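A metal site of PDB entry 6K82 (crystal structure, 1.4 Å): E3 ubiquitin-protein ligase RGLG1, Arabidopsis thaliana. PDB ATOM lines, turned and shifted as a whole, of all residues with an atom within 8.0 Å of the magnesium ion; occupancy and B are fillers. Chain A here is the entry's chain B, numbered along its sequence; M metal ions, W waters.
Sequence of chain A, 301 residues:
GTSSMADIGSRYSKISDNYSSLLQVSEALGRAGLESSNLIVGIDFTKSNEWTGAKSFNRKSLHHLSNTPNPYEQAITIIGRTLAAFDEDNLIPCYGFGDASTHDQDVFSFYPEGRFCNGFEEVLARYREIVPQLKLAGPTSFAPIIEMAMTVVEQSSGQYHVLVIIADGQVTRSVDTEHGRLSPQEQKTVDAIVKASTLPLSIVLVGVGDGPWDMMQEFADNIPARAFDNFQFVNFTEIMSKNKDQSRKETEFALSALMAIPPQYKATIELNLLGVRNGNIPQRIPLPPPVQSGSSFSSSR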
ATOM      1  N   ASP A  44       1.453 -21.776   2.195  1.00  0.00           N
ATOM      2  CA  ASP A  44       2.091 -20.486   1.959  1.00  0.00           C
ATOM      3  C   ASP A  44       3.436 -20.390   2.693  1.00  0.00           C
ATOM      4  O   ASP A  44       3.468 -20.435   3.927  1.00  0.00           O
ATOM      5  CB  ASP A  44       1.117 -19.403   2.436  1.00  0.00           C
ATOM      6  CG  ASP A  44       1.633 -17.974   2.275  1.00  0.00           C
ATOM      7  OD1 ASP A  44       2.843 -17.685   2.486  1.00  0.00           O
ATOM      8  OD2 ASP A  44       0.770 -17.120   1.984  1.00  0.00           O
ATOM      9  N   PHE A  45       4.515 -20.275   1.922  1.00  0.00           N
ATOM     10  CA  PHE A  45       5.861 -20.128   2.479  1.00  0.00           C
ATOM     11  C   PHE A  45       6.441 -18.756   2.104  1.00  0.00           C
ATOM     12  O   PHE A  45       7.635 -18.618   1.798  1.00  0.00           O
ATOM     13  CB  PHE A  45       6.777 -21.258   2.003  1.00  0.00           C
ATOM     14  CG  PHE A  45       6.445 -22.588   2.609  1.00  0.00           C
ATOM     15  CD1 PHE A  45       6.591 -22.798   3.968  1.00  0.00           C
ATOM     16  CD2 PHE A  45       5.985 -23.635   1.812  1.00  0.00           C
ATOM     17  CE1 PHE A  45       6.278 -24.034   4.531  1.00  0.00           C
ATOM     18  CE2 PHE A  45       5.680 -24.852   2.365  1.00  0.00           C
ATOM     19  CZ  PHE A  45       5.826 -25.063   3.724  1.00  0.00           C
ATOM     20  N   THR A  46       5.584 -17.738   2.131  1.00  0.00           N
ATOM     21  CA  THR A  46       6.073 -16.380   1.875  1.00  0.00           C
ATOM     22  C   THR A  46       6.825 -15.783   3.077  1.00  0.00           C
ATOM     23  O   THR A  46       6.563 -16.157   4.228  1.00  0.00           O
ATOM     24  CB  THR A  46       4.911 -15.412   1.462  1.00  0.00           C
ATOM     25  OG1 THR A  46       3.898 -15.358   2.485  1.00  0.00           O
ATOM     26  CG2 THR A  46       4.306 -15.867   0.148  1.00  0.00           C
ATOM     27  N   LYS A  47       7.731 -14.843   2.802  1.00  0.00           N
ATOM     28  CA  LYS A  47       8.566 -14.260   3.843  1.00  0.00           C
ATOM     29  C   LYS A  47       7.752 -13.463   4.864  1.00  0.00           C
ATOM     30  O   LYS A  47       8.128 -13.367   6.026  1.00  0.00           O
ATOM     31  CB  LYS A  47       9.645 -13.373   3.233  1.00  0.00           C
ATOM     32  CG  LYS A  47      10.717 -12.932   4.218  1.00  0.00           C
ATOM     33  CD  LYS A  47      11.895 -12.340   3.461  1.00  0.00           C
ATOM     34  CE  LYS A  47      13.009 -11.941   4.417  1.00  0.00           C
ATOM     35  NZ  LYS A  47      12.603 -10.809   5.278  1.00  0.00           N
ATOM     36  N   SER A  48       6.599 -12.938   4.440  1.00  0.00           N
ATOM     37  CA  SER A  48       5.723 -12.206   5.340  1.00  0.00           C
ATOM     38  C   SER A  48       5.379 -12.992   6.603  1.00  0.00           C
ATOM     39  O   SER A  48       5.049 -12.401   7.628  1.00  0.00           O
ATOM     40  CB  SER A  48       4.434 -11.824   4.634  1.00  0.00           C
ATOM     41  OG  SER A  48       3.725 -13.011   4.332  1.00  0.00           O
ATOM     42  N   ASN A  49       5.424 -14.319   6.517  1.00  0.00           N
ATOM     43  CA  ASN A  49       5.144 -15.168   7.667  1.00  0.00           C
ATOM     44  C   ASN A  49       5.995 -14.825   8.877  1.00  0.00           C
ATOM     45  O   ASN A  49       5.593 -15.069  10.014  1.00  0.00           O
ATOM     46  CB  ASN A  49       5.345 -16.644   7.310  1.00  0.00           C
ATOM     47  CG  ASN A  49       4.138 -17.229   6.598  1.00  0.00           C
ATOM     48  OD1 ASN A  49       3.086 -17.442   7.206  1.00  0.00           O
ATOM     49  ND2 ASN A  49       4.282 -17.487   5.299  1.00  0.00           N
ATOM     50  N   GLU A  50       7.182 -14.268   8.619  1.00  0.00           N
ATOM     51  CA  GLU A  50       8.081 -13.831   9.681  1.00  0.00           C
ATOM     52  C   GLU A  50       7.444 -12.759  10.559  1.00  0.00           C
ATOM     53  O   GLU A  50       7.724 -12.706  11.757  1.00  0.00           O
ATOM     54  CB  GLU A  50       9.401 -13.319   9.084  1.00  0.00           C
ATOM     55  CG  GLU A  50      10.248 -14.394   8.408  1.00  0.00           C
ATOM     56  CD  GLU A  50      11.491 -13.826   7.713  1.00  0.00           C
ATOM     57  OE1 GLU A  50      12.338 -14.642   7.292  1.00  0.00           O
ATOM     58  OE2 GLU A  50      11.609 -12.586   7.583  1.00  0.00           O
ATOM     59  N   TRP A  51       6.608 -11.909   9.993  1.00  0.00           N
ATOM     60  CA  TRP A  51       6.062 -10.814  10.803  1.00  0.00           C
ATOM     61  C   TRP A  51       4.541 -10.776  10.956  1.00  0.00           C
ATOM     62  O   TRP A  51       4.023  -9.964  11.707  1.00  0.00           O
ATOM     63  CB  TRP A  51       6.527  -9.466  10.265  1.00  0.00           C
ATOM     64  CG  TRP A  51       6.619  -9.374   8.782  1.00  0.00           C
ATOM     65  CD1 TRP A  51       7.700  -9.700   8.010  1.00  0.00           C
ATOM     66  CD2 TRP A  51       5.609  -8.904   7.885  1.00  0.00           C
ATOM     67  NE1 TRP A  51       7.414  -9.463   6.688  1.00  0.00           N
ATOM     68  CE2 TRP A  51       6.131  -8.975   6.586  1.00  0.00           C
ATOM     69  CE3 TRP A  51       4.299  -8.435   8.057  1.00  0.00           C
ATOM     70  CZ2 TRP A  51       5.412  -8.601   5.460  1.00  0.00           C
ATOM     71  CZ3 TRP A  51       3.567  -8.066   6.941  1.00  0.00           C
ATOM     72  CH2 TRP A  51       4.131  -8.148   5.658  1.00  0.00           C
ATOM     73  N   THR A  52       3.828 -11.663  10.268  1.00  0.00           N
ATOM     74  CA  THR A  52       2.379 -11.649  10.381  1.00  0.00           C
ATOM     75  C   THR A  52       1.886 -12.370  11.635  1.00  0.00           C
ATOM     76  O   THR A  52       0.686 -12.556  11.826  1.00  0.00           O
ATOM     77  CB  THR A  52       1.704 -12.286   9.148  1.00  0.00           C
ATOM     78  OG1 THR A  52       2.301 -13.565   8.881  1.00  0.00           O
ATOM     79  CG2 THR A  52       1.856 -11.379   7.935  1.00  0.00           C
ATOM     80  N   LEU A  62       5.005 -17.316  11.782  1.00  0.00           N
ATOM     81  CA  LEU A  62       3.912 -18.267  11.670  1.00  0.00           C
ATOM     82  C   LEU A  62       4.418 -19.666  11.351  1.00  0.00           C
ATOM     83  O   LEU A  62       3.709 -20.649  11.572  1.00  0.00           O
ATOM     84  CB  LEU A  62       2.907 -17.827  10.609  1.00  0.00           C
ATOM     85  CG  LEU A  62       2.175 -16.510  10.832  1.00  0.00           C
ATOM     86  CD1 LEU A  62       1.092 -16.378   9.770  1.00  0.00           C
ATOM     87  CD2 LEU A  62       1.577 -16.460  12.227  1.00  0.00           C
ATOM     88  N   TYR A  72      -0.279 -22.966  11.004  1.00  0.00           N
ATOM     89  CA  TYR A  72      -0.354 -23.929   9.904  1.00  0.00           C
ATOM     90  C   TYR A  72      -0.590 -25.349  10.402  1.00  0.00           C
ATOM     91  O   TYR A  72      -1.467 -26.057   9.898  1.00  0.00           O
ATOM     92  CB  TYR A  72       0.933 -23.874   9.056  1.00  0.00           C
ATOM     93  CG  TYR A  72       1.026 -22.605   8.265  1.00  0.00           C
ATOM     94  CD1 TYR A  72       0.466 -22.522   6.996  1.00  0.00           C
ATOM     95  CD2 TYR A  72       1.649 -21.473   8.793  1.00  0.00           C
ATOM     96  CE1 TYR A  72       0.523 -21.338   6.262  1.00  0.00           C
ATOM     97  CE2 TYR A  72       1.712 -20.281   8.069  1.00  0.00           C
ATOM     98  CZ  TYR A  72       1.152 -20.221   6.807  1.00  0.00           C
ATOM     99  OH  TYR A  72       1.234 -19.039   6.091  1.00  0.00           O
ATOM    100  N   PHE A  97       4.133 -23.115  -1.773  1.00  0.00           N
ATOM    101  CA  PHE A  97       4.288 -22.050  -2.750  1.00  0.00           C
ATOM    102  C   PHE A  97       4.722 -20.783  -2.040  1.00  0.00           C
ATOM    103  O   PHE A  97       4.469 -20.622  -0.840  1.00  0.00           O
ATOM    104  CB  PHE A  97       2.983 -21.816  -3.508  1.00  0.00           C
ATOM    105  CG  PHE A  97       1.828 -21.400  -2.630  1.00  0.00           C
ATOM    106  CD1 PHE A  97       1.590 -20.060  -2.362  1.00  0.00           C
ATOM    107  CD2 PHE A  97       0.988 -22.341  -2.059  1.00  0.00           C
ATOM    108  CE1 PHE A  97       0.542 -19.663  -1.547  1.00  0.00           C
ATOM    109  CE2 PHE A  97      -0.079 -21.935  -1.241  1.00  0.00           C
ATOM    110  CZ  PHE A  97      -0.292 -20.584  -0.995  1.00  0.00           C
ATOM    111  N   GLY A  98       5.404 -19.889  -2.761  1.00  0.00           N
ATOM    112  CA  GLY A  98       5.779 -18.608  -2.196  1.00  0.00           C
ATOM    113  C   GLY A  98       7.166 -18.574  -1.582  1.00  0.00           C
ATOM    114  O   GLY A  98       7.614 -17.517  -1.136  1.00  0.00           O
ATOM    115  N   ALA A 137       9.873 -16.386   0.452  1.00  0.00           N
ATOM    116  CA  ALA A 137       9.908 -15.294  -0.511  1.00  0.00           C
ATOM    117  C   ALA A 137       8.513 -14.707  -0.794  1.00  0.00           C
ATOM    118  O   ALA A 137       7.776 -14.351   0.128  1.00  0.00           O
ATOM    119  CB  ALA A 137      10.558 -15.758  -1.808  1.00  0.00           C
ATOM    120  N   GLY A 138       8.150 -14.590  -2.069  1.00  0.00           N
ATOM    121  CA  GLY A 138       6.870 -14.034  -2.468  1.00  0.00           C
ATOM    122  C   GLY A 138       6.898 -13.796  -3.972  1.00  0.00           C
ATOM    123  O   GLY A 138       7.780 -14.315  -4.651  1.00  0.00           O
ATOM    124  N   PRO A 139       5.930 -13.035  -4.503  1.00  0.00           N
ATOM    125  CA  PRO A 139       4.766 -12.494  -3.825  1.00  0.00           C
ATOM    126  C   PRO A 139       3.654 -13.554  -3.763  1.00  0.00           C
ATOM    127  O   PRO A 139       3.964 -14.751  -3.802  1.00  0.00           O
ATOM    128  CB  PRO A 139       4.367 -11.315  -4.717  1.00  0.00           C
ATOM    129  CG  PRO A 139       4.689 -11.819  -6.106  1.00  0.00           C
ATOM    130  CD  PRO A 139       5.930 -12.694  -5.945  1.00  0.00           C
ATOM    131  N   THR A 140       2.399 -13.133  -3.671  1.00  0.00           N
ATOM    132  CA  THR A 140       1.304 -14.065  -3.397  1.00  0.00           C
ATOM    133  C   THR A 140       0.317 -14.205  -4.554  1.00  0.00           C
ATOM    134  O   THR A 140      -0.386 -13.263  -4.913  1.00  0.00           O
ATOM    135  CB  THR A 140       0.558 -13.652  -2.116  1.00  0.00           C
ATOM    136  OG1 THR A 140       1.479 -13.577  -1.029  1.00  0.00           O
ATOM    137  CG2 THR A 140      -0.555 -14.678  -1.788  1.00  0.00           C
ATOM    138  N   PHE A 142      -2.574 -17.375  -5.874  1.00  0.00           N
ATOM    139  CA  PHE A 142      -3.092 -18.739  -5.646  1.00  0.00           C
ATOM    140  C   PHE A 142      -3.363 -19.446  -6.966  1.00  0.00           C
ATOM    141  O   PHE A 142      -3.862 -20.573  -6.970  1.00  0.00           O
ATOM    142  CB  PHE A 142      -4.342 -18.714  -4.744  1.00  0.00           C
ATOM    143  CG  PHE A 142      -4.117 -18.029  -3.422  1.00  0.00           C
ATOM    144  CD1 PHE A 142      -2.979 -18.323  -2.662  1.00  0.00           C
ATOM    145  CD2 PHE A 142      -4.981 -17.059  -2.965  1.00  0.00           C
ATOM    146  CE1 PHE A 142      -2.742 -17.672  -1.455  1.00  0.00           C
ATOM    147  CE2 PHE A 142      -4.750 -16.393  -1.776  1.00  0.00           C
ATOM    148  CZ  PHE A 142      -3.626 -16.692  -1.016  1.00  0.00           C
ATOM    149  N   ALA A 167      -2.817 -19.708   4.036  1.00  0.00           N
ATOM    150  CA  ALA A 167      -2.043 -18.557   3.591  1.00  0.00           C
ATOM    151  C   ALA A 167      -2.044 -17.462   4.640  1.00  0.00           C
ATOM    152  O   ALA A 167      -2.964 -17.368   5.456  1.00  0.00           O
ATOM    153  CB  ALA A 167      -2.584 -18.020   2.261  1.00  0.00           C
ATOM    154  N   ASP A 168      -1.013 -16.608   4.588  1.00  0.00           N
ATOM    155  CA  ASP A 168      -0.925 -15.486   5.530  1.00  0.00           C
ATOM    156  C   ASP A 168      -1.163 -14.130   4.881  1.00  0.00           C
ATOM    157  O   ASP A 168      -0.918 -13.099   5.506  1.00  0.00           O
ATOM    158  CB  ASP A 168       0.437 -15.489   6.263  1.00  0.00           C
ATOM    159  CG  ASP A 168       1.531 -14.773   5.495  1.00  0.00           C
ATOM    160  OD1 ASP A 168       1.524 -14.786   4.244  1.00  0.00           O
ATOM    161  OD2 ASP A 168       2.419 -14.179   6.159  1.00  0.00           O
ATOM    162  N   GLY A 169      -1.632 -14.118   3.636  1.00  0.00           N
ATOM    163  CA  GLY A 169      -2.011 -12.848   3.023  1.00  0.00           C
ATOM    164  C   GLY A 169      -2.984 -12.984   1.875  1.00  0.00           C
ATOM    165  O   GLY A 169      -3.127 -14.069   1.285  1.00  0.00           O
ATOM    166  N   GLN A 170      -3.646 -11.884   1.547  1.00  0.00           N
ATOM    167  CA  GLN A 170      -4.466 -11.793   0.344  1.00  0.00           C
ATOM    168  C   GLN A 170      -3.596 -11.911  -0.892  1.00  0.00           C
ATOM    169  O   GLN A 170      -2.371 -11.793  -0.830  1.00  0.00           O
ATOM    170  CB  GLN A 170      -5.235 -10.459   0.331  1.00  0.00           C
ATOM    171  CG  GLN A 170      -4.302  -9.266   0.127  1.00  0.00           C
ATOM    172  CD  GLN A 170      -4.985  -7.917   0.338  1.00  0.00           C
ATOM    173  OE1 GLN A 170      -6.209  -7.811   0.276  1.00  0.00           O
ATOM    174  NE2 GLN A 170      -4.185  -6.889   0.586  1.00  0.00           N
ATOM    175  N   THR A 172      -1.618 -10.726  -3.934  1.00  0.00           N
ATOM    176  CA  THR A 172      -0.900  -9.467  -4.131  1.00  0.00           C
ATOM    177  C   THR A 172      -1.712  -8.526  -5.004  1.00  0.00           C
ATOM    178  O   THR A 172      -2.197  -8.907  -6.071  1.00  0.00           O
ATOM    179  CB  THR A 172       0.455  -9.750  -4.723  1.00  0.00           C
ATOM    180  OG1 THR A 172       1.242 -10.457  -3.756  1.00  0.00           O
ATOM    181  CG2 THR A 172       1.172  -8.438  -5.117  1.00  0.00           C
ATOM    182  N   VAL A 208      -4.370 -17.397   7.972  1.00  0.00           N
ATOM    183  CA  VAL A 208      -3.729 -17.445   9.277  1.00  0.00           C
ATOM    184  C   VAL A 208      -2.957 -16.151   9.482  1.00  0.00           C
ATOM    185  O   VAL A 208      -2.699 -15.401   8.537  1.00  0.00           O
ATOM    186  CB  VAL A 208      -2.784 -18.673   9.425  1.00  0.00           C
ATOM    187  CG1 VAL A 208      -3.589 -19.967   9.385  1.00  0.00           C
ATOM    188  CG2 VAL A 208      -1.719 -18.650   8.334  1.00  0.00           C
ATOM    189  N   GLY A 211      -3.023 -10.885   8.873  1.00  0.00           N
ATOM    190  CA  GLY A 211      -3.549 -10.348   7.642  1.00  0.00           C
ATOM    191  C   GLY A 211      -2.799  -9.106   7.178  1.00  0.00           C
ATOM    192  O   GLY A 211      -1.564  -9.122   7.086  1.00  0.00           O
ATOM    193  N   TRP A 213      -7.041  -8.959   6.629  1.00  0.00           N
ATOM    194  CA  TRP A 213      -7.954  -9.832   5.912  1.00  0.00           C
ATOM    195  C   TRP A 213      -9.254  -9.142   5.528  1.00  0.00           C
ATOM    196  O   TRP A 213     -10.158  -9.779   4.983  1.00  0.00           O
ATOM    197  CB  TRP A 213      -8.264 -11.059   6.778  1.00  0.00           C
ATOM    198  CG  TRP A 213      -7.086 -11.960   6.993  1.00  0.00           C
ATOM    199  CD1 TRP A 213      -6.459 -12.243   8.177  1.00  0.00           C
ATOM    200  CD2 TRP A 213      -6.413 -12.730   5.999  1.00  0.00           C
ATOM    201  NE1 TRP A 213      -5.438 -13.136   7.975  1.00  0.00           N
ATOM    202  CE2 TRP A 213      -5.384 -13.447   6.639  1.00  0.00           C
ATOM    203  CE3 TRP A 213      -6.577 -12.881   4.619  1.00  0.00           C
ATOM    204  CZ2 TRP A 213      -4.528 -14.302   5.952  1.00  0.00           C
ATOM    205  CZ3 TRP A 213      -5.717 -13.727   3.932  1.00  0.00           C
ATOM    206  CH2 TRP A 213      -4.707 -14.424   4.606  1.00  0.00           C
HETATM  207 MG    MG M   1       2.508 -13.692   2.795  1.00  0.00          MG
HETATM  208  O   HOH W   1       1.235 -12.098   3.076  1.00  0.00           O
HETATM  209  O   HOH W   2       3.608 -12.568   1.337  1.00  0.00           O
HETATM  210  O   HOH W   3       1.181 -14.550   1.444  1.00  0.00           O
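Water W3 bridges the side-chain carboxylate of Asp 44 (2.7 Å) and the side-chain hydroxyl of Thr 140 (2.7 Å).
OD1 of Asp 44 is in hydrogen-bond range of ND2 of Asn 49 (3.2 Å).
The side-chain carboxylate (OD2) of Asp 44 lies within hydrogen-bond range of the backbone NH (N) of Asp 168, 3.2 Å away.
The side-chain amide nitrogen (ND2) of Asn 49 lies within hydrogen-bond range of the backbone carbonyl oxygen (O) of Thr 46, 2.8 Å away.
N of Asn 49 sits at hydrogen-bond distance from OD2 of Asp 168, 3.0 Å away.
N of Thr 46 is in hydrogen-bond range of OD1 of Asp 44 (2.8 Å).
The side-chain hydroxyl (OH) of Tyr 72 is in hydrogen-bond range of the backbone carbonyl oxygen (O) of Asp 44 (3.4 Å).
OD2 of Asp 168 is in hydrogen-bond range of OG1 of Thr 52 (2.8 Å).
O of Ser 48 is in hydrogen-bond range of OG1 of Thr 52, 3.2 Å away.
The magnesium ion is bound by water W1 (2.1 Å), OD1 of Asp 168 (2.1 Å), OG of Ser 48 (2.1 Å), water W3 (2.1 Å), water W2 (2.1 Å) and OG1 of Thr 46 (2.2 Å).
Merely in contact with the magnesium ion: Asp 44 and Thr 140.
Of the 26 residues printed, 5 come within 4 Å of the magnesium ion.
The nearest printed residue that does not touch the magnesium ion is Gly 169 (4.2 Å).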
